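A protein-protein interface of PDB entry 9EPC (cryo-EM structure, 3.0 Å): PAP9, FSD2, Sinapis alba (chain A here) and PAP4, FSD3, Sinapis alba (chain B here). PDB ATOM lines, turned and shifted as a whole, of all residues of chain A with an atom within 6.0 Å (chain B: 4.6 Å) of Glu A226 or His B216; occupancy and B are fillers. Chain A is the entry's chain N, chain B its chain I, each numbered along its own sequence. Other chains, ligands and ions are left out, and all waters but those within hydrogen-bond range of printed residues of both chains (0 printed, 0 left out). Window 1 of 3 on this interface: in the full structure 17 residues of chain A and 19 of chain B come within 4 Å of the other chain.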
ATOM      1  N   GLY A 170       2.148  25.496  -2.438  1.00  0.00           N
ATOM      2  CA  GLY A 170       1.459  24.753  -1.407  1.00  0.00           C
ATOM      3  C   GLY A 170       0.395  23.828  -1.974  1.00  0.00           C
ATOM      4  O   GLY A 170       0.344  23.533  -3.171  1.00  0.00           O
ATOM      5  N   SER A 171      -0.470  23.365  -1.077  1.00  0.00           N
ATOM      6  CA  SER A 171      -1.563  22.478  -1.445  1.00  0.00           C
ATOM      7  C   SER A 171      -2.763  23.303  -1.889  1.00  0.00           C
ATOM      8  O   SER A 171      -3.204  24.205  -1.171  1.00  0.00           O
ATOM      9  CB  SER A 171      -1.942  21.573  -0.273  1.00  0.00           C
ATOM     10  OG  SER A 171      -2.256  22.338   0.876  1.00  0.00           O
ATOM     11  N   ASP A 223      -5.924  18.233  -9.341  1.00  0.00           N
ATOM     12  CA  ASP A 223      -5.618  18.163  -7.920  1.00  0.00           C
ATOM     13  C   ASP A 223      -4.134  18.409  -7.692  1.00  0.00           C
ATOM     14  O   ASP A 223      -3.329  17.474  -7.743  1.00  0.00           O
ATOM     15  CB  ASP A 223      -6.033  16.807  -7.343  1.00  0.00           C
ATOM     16  CG  ASP A 223      -6.007  16.784  -5.827  1.00  0.00           C
ATOM     17  OD1 ASP A 223      -5.805  17.854  -5.218  1.00  0.00           O
ATOM     18  OD2 ASP A 223      -6.193  15.697  -5.244  1.00  0.00           O
ATOM     19  N   THR A 224      -3.765  19.662  -7.435  1.00  0.00           N
ATOM     20  CA  THR A 224      -2.369  20.010  -7.208  1.00  0.00           C
ATOM     21  C   THR A 224      -1.925  19.754  -5.777  1.00  0.00           C
ATOM     22  O   THR A 224      -0.768  20.039  -5.447  1.00  0.00           O
ATOM     23  CB  THR A 224      -2.119  21.474  -7.577  1.00  0.00           C
ATOM     24  OG1 THR A 224      -3.176  22.288  -7.058  1.00  0.00           O
ATOM     25  CG2 THR A 224      -2.058  21.637  -9.087  1.00  0.00           C
ATOM     26  N   TRP A 225      -2.810  19.244  -4.925  1.00  0.00           N
ATOM     27  CA  TRP A 225      -2.393  18.755  -3.620  1.00  0.00           C
ATOM     28  C   TRP A 225      -1.326  17.683  -3.788  1.00  0.00           C
ATOM     29  O   TRP A 225      -1.411  16.838  -4.681  1.00  0.00           O
ATOM     30  CB  TRP A 225      -3.587  18.187  -2.858  1.00  0.00           C
ATOM     31  CG  TRP A 225      -4.441  19.213  -2.198  1.00  0.00           C
ATOM     32  CD1 TRP A 225      -5.122  20.224  -2.802  1.00  0.00           C
ATOM     33  CD2 TRP A 225      -4.727  19.314  -0.800  1.00  0.00           C
ATOM     34  NE1 TRP A 225      -5.807  20.959  -1.866  1.00  0.00           N
ATOM     35  CE2 TRP A 225      -5.581  20.419  -0.627  1.00  0.00           C
ATOM     36  CE3 TRP A 225      -4.340  18.580   0.324  1.00  0.00           C
ATOM     37  CZ2 TRP A 225      -6.054  20.807   0.622  1.00  0.00           C
ATOM     38  CZ3 TRP A 225      -4.809  18.967   1.562  1.00  0.00           C
ATOM     39  CH2 TRP A 225      -5.658  20.069   1.702  1.00  0.00           C
ATOM     40  N   GLU A 226      -0.312  17.727  -2.922  1.00  0.00           N
ATOM     41  CA  GLU A 226       0.820  16.820  -3.073  1.00  0.00           C
ATOM     42  C   GLU A 226       0.395  15.361  -2.976  1.00  0.00           C
ATOM     43  O   GLU A 226       0.974  14.506  -3.654  1.00  0.00           O
ATOM     44  CB  GLU A 226       1.888  17.139  -2.028  1.00  0.00           C
ATOM     45  CG  GLU A 226       2.500  18.521  -2.182  1.00  0.00           C
ATOM     46  CD  GLU A 226       3.560  18.810  -1.140  1.00  0.00           C
ATOM     47  OE1 GLU A 226       3.623  18.077  -0.132  1.00  0.00           O
ATOM     48  OE2 GLU A 226       4.332  19.772  -1.330  1.00  0.00           O
ATOM     49  N   HIS A 227      -0.621  15.057  -2.165  1.00  0.00           N
ATOM     50  CA  HIS A 227      -1.055  13.672  -2.018  1.00  0.00           C
ATOM     51  C   HIS A 227      -1.513  13.082  -3.344  1.00  0.00           C
ATOM     52  O   HIS A 227      -1.449  11.863  -3.537  1.00  0.00           O
ATOM     53  CB  HIS A 227      -2.176  13.574  -0.983  1.00  0.00           C
ATOM     54  CG  HIS A 227      -3.448  14.244  -1.400  1.00  0.00           C
ATOM     55  ND1 HIS A 227      -4.294  13.714  -2.350  1.00  0.00           N
ATOM     56  CD2 HIS A 227      -4.024  15.397  -0.987  1.00  0.00           C
ATOM     57  CE1 HIS A 227      -5.332  14.516  -2.510  1.00  0.00           C
ATOM     58  NE2 HIS A 227      -5.193  15.545  -1.695  1.00  0.00           N
ATOM     59  N   ALA A 228      -1.974  13.927  -4.267  1.00  0.00           N
ATOM     60  CA  ALA A 228      -2.488  13.428  -5.536  1.00  0.00           C
ATOM     61  C   ALA A 228      -1.381  12.880  -6.426  1.00  0.00           C
ATOM     62  O   ALA A 228      -1.628  11.973  -7.228  1.00  0.00           O
ATOM     63  CB  ALA A 228      -3.248  14.535  -6.264  1.00  0.00           C
ATOM     64  N   TYR A 229      -0.165  13.408  -6.305  1.00  0.00           N
ATOM     65  CA  TYR A 229       0.885  13.063  -7.254  1.00  0.00           C
ATOM     66  C   TYR A 229       2.240  12.761  -6.638  1.00  0.00           C
ATOM     67  O   TYR A 229       3.136  12.338  -7.374  1.00  0.00           O
ATOM     68  CB  TYR A 229       1.059  14.197  -8.272  1.00  0.00           C
ATOM     69  CG  TYR A 229       1.587  15.484  -7.677  1.00  0.00           C
ATOM     70  CD1 TYR A 229       0.733  16.391  -7.065  1.00  0.00           C
ATOM     71  CD2 TYR A 229       2.940  15.794  -7.733  1.00  0.00           C
ATOM     72  CE1 TYR A 229       1.210  17.567  -6.522  1.00  0.00           C
ATOM     73  CE2 TYR A 229       3.425  16.969  -7.193  1.00  0.00           C
ATOM     74  CZ  TYR A 229       2.556  17.851  -6.589  1.00  0.00           C
ATOM     75  OH  TYR A 229       3.034  19.022  -6.049  1.00  0.00           O
ATOM     76  N   TYR A 230       2.437  12.959  -5.335  1.00  0.00           N
ATOM     77  CA  TYR A 230       3.781  12.843  -4.782  1.00  0.00           C
ATOM     78  C   TYR A 230       4.232  11.395  -4.674  1.00  0.00           C
ATOM     79  O   TYR A 230       5.436  11.118  -4.712  1.00  0.00           O
ATOM     80  CB  TYR A 230       3.846  13.512  -3.412  1.00  0.00           C
ATOM     81  CG  TYR A 230       5.249  13.722  -2.916  1.00  0.00           C
ATOM     82  CD1 TYR A 230       6.024  14.760  -3.405  1.00  0.00           C
ATOM     83  CD2 TYR A 230       5.801  12.885  -1.958  1.00  0.00           C
ATOM     84  CE1 TYR A 230       7.306  14.959  -2.958  1.00  0.00           C
ATOM     85  CE2 TYR A 230       7.087  13.080  -1.503  1.00  0.00           C
ATOM     86  CZ  TYR A 230       7.835  14.119  -2.007  1.00  0.00           C
ATOM     87  OH  TYR A 230       9.120  14.321  -1.559  1.00  0.00           O
ATOM     88  N   LEU A 231       3.290  10.461  -4.543  1.00  0.00           N
ATOM     89  CA  LEU A 231       3.651   9.096  -4.183  1.00  0.00           C
ATOM     90  C   LEU A 231       4.345   8.357  -5.319  1.00  0.00           C
ATOM     91  O   LEU A 231       5.252   7.557  -5.064  1.00  0.00           O
ATOM     92  CB  LEU A 231       2.407   8.333  -3.730  1.00  0.00           C
ATOM     93  CG  LEU A 231       2.624   6.930  -3.160  1.00  0.00           C
ATOM     94  CD1 LEU A 231       3.651   6.956  -2.040  1.00  0.00           C
ATOM     95  CD2 LEU A 231       1.310   6.356  -2.665  1.00  0.00           C
ATOM     96  N   ARG A 237       6.144  17.711 -10.054  1.00  0.00           N
ATOM     97  CA  ARG A 237       4.814  18.220 -10.368  1.00  0.00           C
ATOM     98  C   ARG A 237       4.687  18.548 -11.848  1.00  0.00           C
ATOM     99  O   ARG A 237       3.593  18.444 -12.414  1.00  0.00           O
ATOM    100  CB  ARG A 237       4.511  19.454  -9.517  1.00  0.00           C
ATOM    101  CG  ARG A 237       3.150  20.082  -9.784  1.00  0.00           C
ATOM    102  CD  ARG A 237       2.946  21.354  -8.974  1.00  0.00           C
ATOM    103  NE  ARG A 237       2.839  21.091  -7.544  1.00  0.00           N
ATOM    104  CZ  ARG A 237       2.579  22.017  -6.630  1.00  0.00           C
ATOM    105  NH1 ARG A 237       2.394  23.285  -6.962  1.00  0.00           N
ATOM    106  NH2 ARG A 237       2.502  21.663  -5.351  1.00  0.00           N
ATOM    107  N   THR B  71      13.194   9.491   1.044  1.00  0.00           N
ATOM    108  CA  THR B  71      12.344  10.665   1.207  1.00  0.00           C
ATOM    109  C   THR B  71      13.172  11.888   1.581  1.00  0.00           C
ATOM    110  O   THR B  71      12.839  13.015   1.200  1.00  0.00           O
ATOM    111  CB  THR B  71      11.274  10.395   2.261  1.00  0.00           C
ATOM    112  OG1 THR B  71      10.691   9.108   2.024  1.00  0.00           O
ATOM    113  CG2 THR B  71      10.183  11.455   2.191  1.00  0.00           C
ATOM    114  N   HIS B  75      13.020  15.423  -0.221  1.00  0.00           N
ATOM    115  CA  HIS B  75      12.577  16.534   0.615  1.00  0.00           C
ATOM    116  C   HIS B  75      13.677  17.578   0.763  1.00  0.00           C
ATOM    117  O   HIS B  75      13.428  18.782   0.652  1.00  0.00           O
ATOM    118  CB  HIS B  75      12.136  16.016   1.984  1.00  0.00           C
ATOM    119  CG  HIS B  75      11.509  17.061   2.854  1.00  0.00           C
ATOM    120  ND1 HIS B  75      11.145  16.818   4.161  1.00  0.00           N
ATOM    121  CD2 HIS B  75      11.174  18.348   2.604  1.00  0.00           C
ATOM    122  CE1 HIS B  75      10.618  17.912   4.679  1.00  0.00           C
ATOM    123  NE2 HIS B  75      10.623  18.856   3.756  1.00  0.00           N
ATOM    124  N   HIS B  79      13.094  19.501  -2.932  1.00  0.00           N
ATOM    125  CA  HIS B  79      12.262  20.599  -2.452  1.00  0.00           C
ATOM    126  C   HIS B  79      13.112  21.729  -1.892  1.00  0.00           C
ATOM    127  O   HIS B  79      12.944  22.894  -2.270  1.00  0.00           O
ATOM    128  CB  HIS B  79      11.287  20.093  -1.391  1.00  0.00           C
ATOM    129  CG  HIS B  79      10.226  19.188  -1.929  1.00  0.00           C
ATOM    130  ND1 HIS B  79       9.092  19.663  -2.552  1.00  0.00           N
ATOM    131  CD2 HIS B  79      10.125  17.839  -1.936  1.00  0.00           C
ATOM    132  CE1 HIS B  79       8.338  18.643  -2.920  1.00  0.00           C
ATOM    133  NE2 HIS B  79       8.942  17.526  -2.559  1.00  0.00           N
ATOM    134  N   HIS B 128      12.791  25.134   6.077  1.00  0.00           N
ATOM    135  CA  HIS B 128      13.430  23.837   5.884  1.00  0.00           C
ATOM    136  C   HIS B 128      14.755  23.757   6.629  1.00  0.00           C
ATOM    137  O   HIS B 128      15.071  22.723   7.228  1.00  0.00           O
ATOM    138  CB  HIS B 128      13.619  23.559   4.396  1.00  0.00           C
ATOM    139  CG  HIS B 128      12.417  22.951   3.744  1.00  0.00           C
ATOM    140  ND1 HIS B 128      11.200  23.593   3.681  1.00  0.00           N
ATOM    141  CD2 HIS B 128      12.241  21.750   3.143  1.00  0.00           C
ATOM    142  CE1 HIS B 128      10.328  22.819   3.061  1.00  0.00           C
ATOM    143  NE2 HIS B 128      10.934  21.695   2.724  1.00  0.00           N
ATOM    144  N   ASP B 212       7.253  20.036  10.056  1.00  0.00           N
ATOM    145  CA  ASP B 212       6.809  20.187   8.676  1.00  0.00           C
ATOM    146  C   ASP B 212       5.667  19.212   8.426  1.00  0.00           C
ATOM    147  O   ASP B 212       5.878  17.996   8.387  1.00  0.00           O
ATOM    148  CB  ASP B 212       7.963  19.939   7.707  1.00  0.00           C
ATOM    149  CG  ASP B 212       7.613  20.308   6.281  1.00  0.00           C
ATOM    150  OD1 ASP B 212       6.525  20.879   6.068  1.00  0.00           O
ATOM    151  OD2 ASP B 212       8.425  20.031   5.374  1.00  0.00           O
ATOM    152  N   TRP B 214       3.852  19.525   5.625  1.00  0.00           N
ATOM    153  CA  TRP B 214       3.682  19.423   4.184  1.00  0.00           C
ATOM    154  C   TRP B 214       3.632  17.959   3.775  1.00  0.00           C
ATOM    155  O   TRP B 214       4.373  17.125   4.301  1.00  0.00           O
ATOM    156  CB  TRP B 214       4.824  20.132   3.458  1.00  0.00           C
ATOM    157  CG  TRP B 214       4.669  21.615   3.369  1.00  0.00           C
ATOM    158  CD1 TRP B 214       4.576  22.491   4.405  1.00  0.00           C
ATOM    159  CD2 TRP B 214       4.610  22.401   2.174  1.00  0.00           C
ATOM    160  NE1 TRP B 214       4.450  23.773   3.933  1.00  0.00           N
ATOM    161  CE2 TRP B 214       4.471  23.745   2.565  1.00  0.00           C
ATOM    162  CE3 TRP B 214       4.657  22.097   0.811  1.00  0.00           C
ATOM    163  CZ2 TRP B 214       4.376  24.783   1.644  1.00  0.00           C
ATOM    164  CZ3 TRP B 214       4.565  23.127  -0.101  1.00  0.00           C
ATOM    165  CH2 TRP B 214       4.428  24.455   0.318  1.00  0.00           C
ATOM    166  N   GLU B 215       2.750  17.649   2.824  1.00  0.00           N
ATOM    167  CA  GLU B 215       2.549  16.257   2.436  1.00  0.00           C
ATOM    168  C   GLU B 215       3.818  15.640   1.863  1.00  0.00           C
ATOM    169  O   GLU B 215       3.995  14.419   1.931  1.00  0.00           O
ATOM    170  CB  GLU B 215       1.403  16.155   1.431  1.00  0.00           C
ATOM    171  CG  GLU B 215       0.058  16.574   1.997  1.00  0.00           C
ATOM    172  CD  GLU B 215      -1.058  16.489   0.976  1.00  0.00           C
ATOM    173  OE1 GLU B 215      -0.759  16.452  -0.234  1.00  0.00           O
ATOM    174  OE2 GLU B 215      -2.238  16.457   1.387  1.00  0.00           O
ATOM    175  N   HIS B 216       4.717  16.458   1.311  1.00  0.00           N
ATOM    176  CA  HIS B 216       5.960  15.919   0.774  1.00  0.00           C
ATOM    177  C   HIS B 216       6.880  15.394   1.866  1.00  0.00           C
ATOM    178  O   HIS B 216       7.797  14.622   1.567  1.00  0.00           O
ATOM    179  CB  HIS B 216       6.690  16.979  -0.057  1.00  0.00           C
ATOM    180  CG  HIS B 216       7.191  18.148   0.737  1.00  0.00           C
ATOM    181  ND1 HIS B 216       6.784  19.441   0.489  1.00  0.00           N
ATOM    182  CD2 HIS B 216       8.079  18.223   1.756  1.00  0.00           C
ATOM    183  CE1 HIS B 216       7.394  20.260   1.327  1.00  0.00           C
ATOM    184  NE2 HIS B 216       8.182  19.546   2.109  1.00  0.00           N
ATOM    185  N   SER B 217       6.664  15.795   3.117  1.00  0.00           N
ATOM    186  CA  SER B 217       7.567  15.418   4.194  1.00  0.00           C
ATOM    187  C   SER B 217       7.250  14.055   4.794  1.00  0.00           C
ATOM    188  O   SER B 217       8.105  13.486   5.481  1.00  0.00           O
ATOM    189  CB  SER B 217       7.536  16.477   5.297  1.00  0.00           C
ATOM    190  OG  SER B 217       6.224  16.641   5.805  1.00  0.00           O
ATOM    191  N   TYR B 218       6.052  13.520   4.561  1.00  0.00           N
ATOM    192  CA  TYR B 218       5.672  12.268   5.201  1.00  0.00           C
ATOM    193  C   TYR B 218       4.975  11.268   4.293  1.00  0.00           C
ATOM    194  O   TYR B 218       4.797  10.121   4.715  1.00  0.00           O
ATOM    195  CB  TYR B 218       4.763  12.546   6.407  1.00  0.00           C
ATOM    196  CG  TYR B 218       3.498  13.301   6.066  1.00  0.00           C
ATOM    197  CD1 TYR B 218       2.346  12.629   5.679  1.00  0.00           C
ATOM    198  CD2 TYR B 218       3.453  14.686   6.138  1.00  0.00           C
ATOM    199  CE1 TYR B 218       1.189  13.314   5.369  1.00  0.00           C
ATOM    200  CE2 TYR B 218       2.299  15.379   5.831  1.00  0.00           C
ATOM    201  CZ  TYR B 218       1.171  14.689   5.446  1.00  0.00           C
ATOM    202  OH  TYR B 218       0.020  15.376   5.138  1.00  0.00           O
ATOM    203  N   TYR B 219       4.566  11.645   3.080  1.00  0.00           N
ATOM    204  CA  TYR B 219       3.721  10.756   2.289  1.00  0.00           C
ATOM    205  C   TYR B 219       4.468   9.498   1.864  1.00  0.00           C
ATOM    206  O   TYR B 219       3.893   8.405   1.855  1.00  0.00           O
ATOM    207  CB  TYR B 219       3.172  11.490   1.069  1.00  0.00           C
ATOM    208  CG  TYR B 219       1.800  11.011   0.675  1.00  0.00           C
ATOM    209  CD1 TYR B 219       0.670  11.484   1.327  1.00  0.00           C
ATOM    210  CD2 TYR B 219       1.630  10.078  -0.336  1.00  0.00           C
ATOM    211  CE1 TYR B 219      -0.587  11.047   0.979  1.00  0.00           C
ATOM    212  CE2 TYR B 219       0.373   9.635  -0.693  1.00  0.00           C
ATOM    213  CZ  TYR B 219      -0.733  10.124  -0.031  1.00  0.00           C
ATOM    214  OH  TYR B 219      -1.990   9.690  -0.378  1.00  0.00           O
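NE2 of His B79 lies close to OH of Tyr A230 (3.4 Å).
The backbone carbonyl oxygen (O) of His B216 is in hydrogen-bond range of the side-chain hydroxyl (OH) of Tyr A230 (3.4 Å).
OE1 of Glu A226 lies within hydrogen-bond range of N of His B216 (2.4 Å).
The backbone NH of His A227 lies close to the side-chain carboxylate of Glu B215, at 2.4 Å.
The side-chain carboxylate of Glu B215 lies within hydrogen-bond range of the backbone NH of Glu A226 (3.0 Å).
The backbone carbonyl oxygen (O) of Trp B214 lies within hydrogen-bond range of the side-chain hydroxyl (OG) of Ser B217 (2.4 Å).
The side-chain carboxylate (OD1) of Asp B212 lies close to the backbone NH (N) of Trp B214 (3.0 Å).
A ring nitrogen (NE2) of His B216 lies close to a ring nitrogen (NE2) of His B75 (3.0 Å).
OD1 of Asp A223 lies close to N of Trp A225 (3.3 Å).
Among the printed residues, merely in contact across the chains: Gly A170 with Trp B214 (3.4 Å), Trp A225 with Glu B215 (3.2 Å), Glu A226 with Trp B214 (3.2 Å), His A227 with Tyr B219 (3.6 Å) and Leu A231 with Tyr B219 (3.9 Å).
Of the printed residues of chain B, Gly A170 touches Trp B214.
Of the printed residues of chain B, Trp A225 touches Glu B215.
Glu A226 touches just these residues of chain B: Trp B214 (3.2 Å), Glu B215 (3.0 Å) and His B216 (2.4 Å).
Thr B71 touches none of the printed residues of chain A.
Of the printed residues of chain A, Glu B215 touches Trp A225 (3.2 Å), Glu A226 (3.0 Å) and His A227 (2.4 Å).
His B216 touches just these residues of chain A: Glu A226 (2.4 Å) and Tyr A230 (3.4 Å).
Of the printed residues of chain A, Tyr B219 touches His A227 (3.6 Å) and Leu A231 (3.9 Å).
The nearest residue of chain B that does not touch Glu A226 is His B79 (4.5 Å).
The nearest printed residue of chain A that does not touch His B216 is His A227 (6.5 Å).
The nearest printed residue of chain B that does not touch His A227 is His B216 (6.5 Å).
Of the 11 printed residues of chain B, 5 touch a printed residue of chain A.
Hydrophobic or aromatic side chains of chain B within 4 Å of the printed part of chain A: His B79, Trp B214, His B216 and Tyr B219.
Of the 12 printed residues of chain A, 6 touch a printed residue of chain B.
Among the printed residues, 10 pairs touch across the chains.
Among the printed residues, no Asp or Glu carboxylate lies within 4 Å of a Lys or Arg side-chain nitrogen of the other chain.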
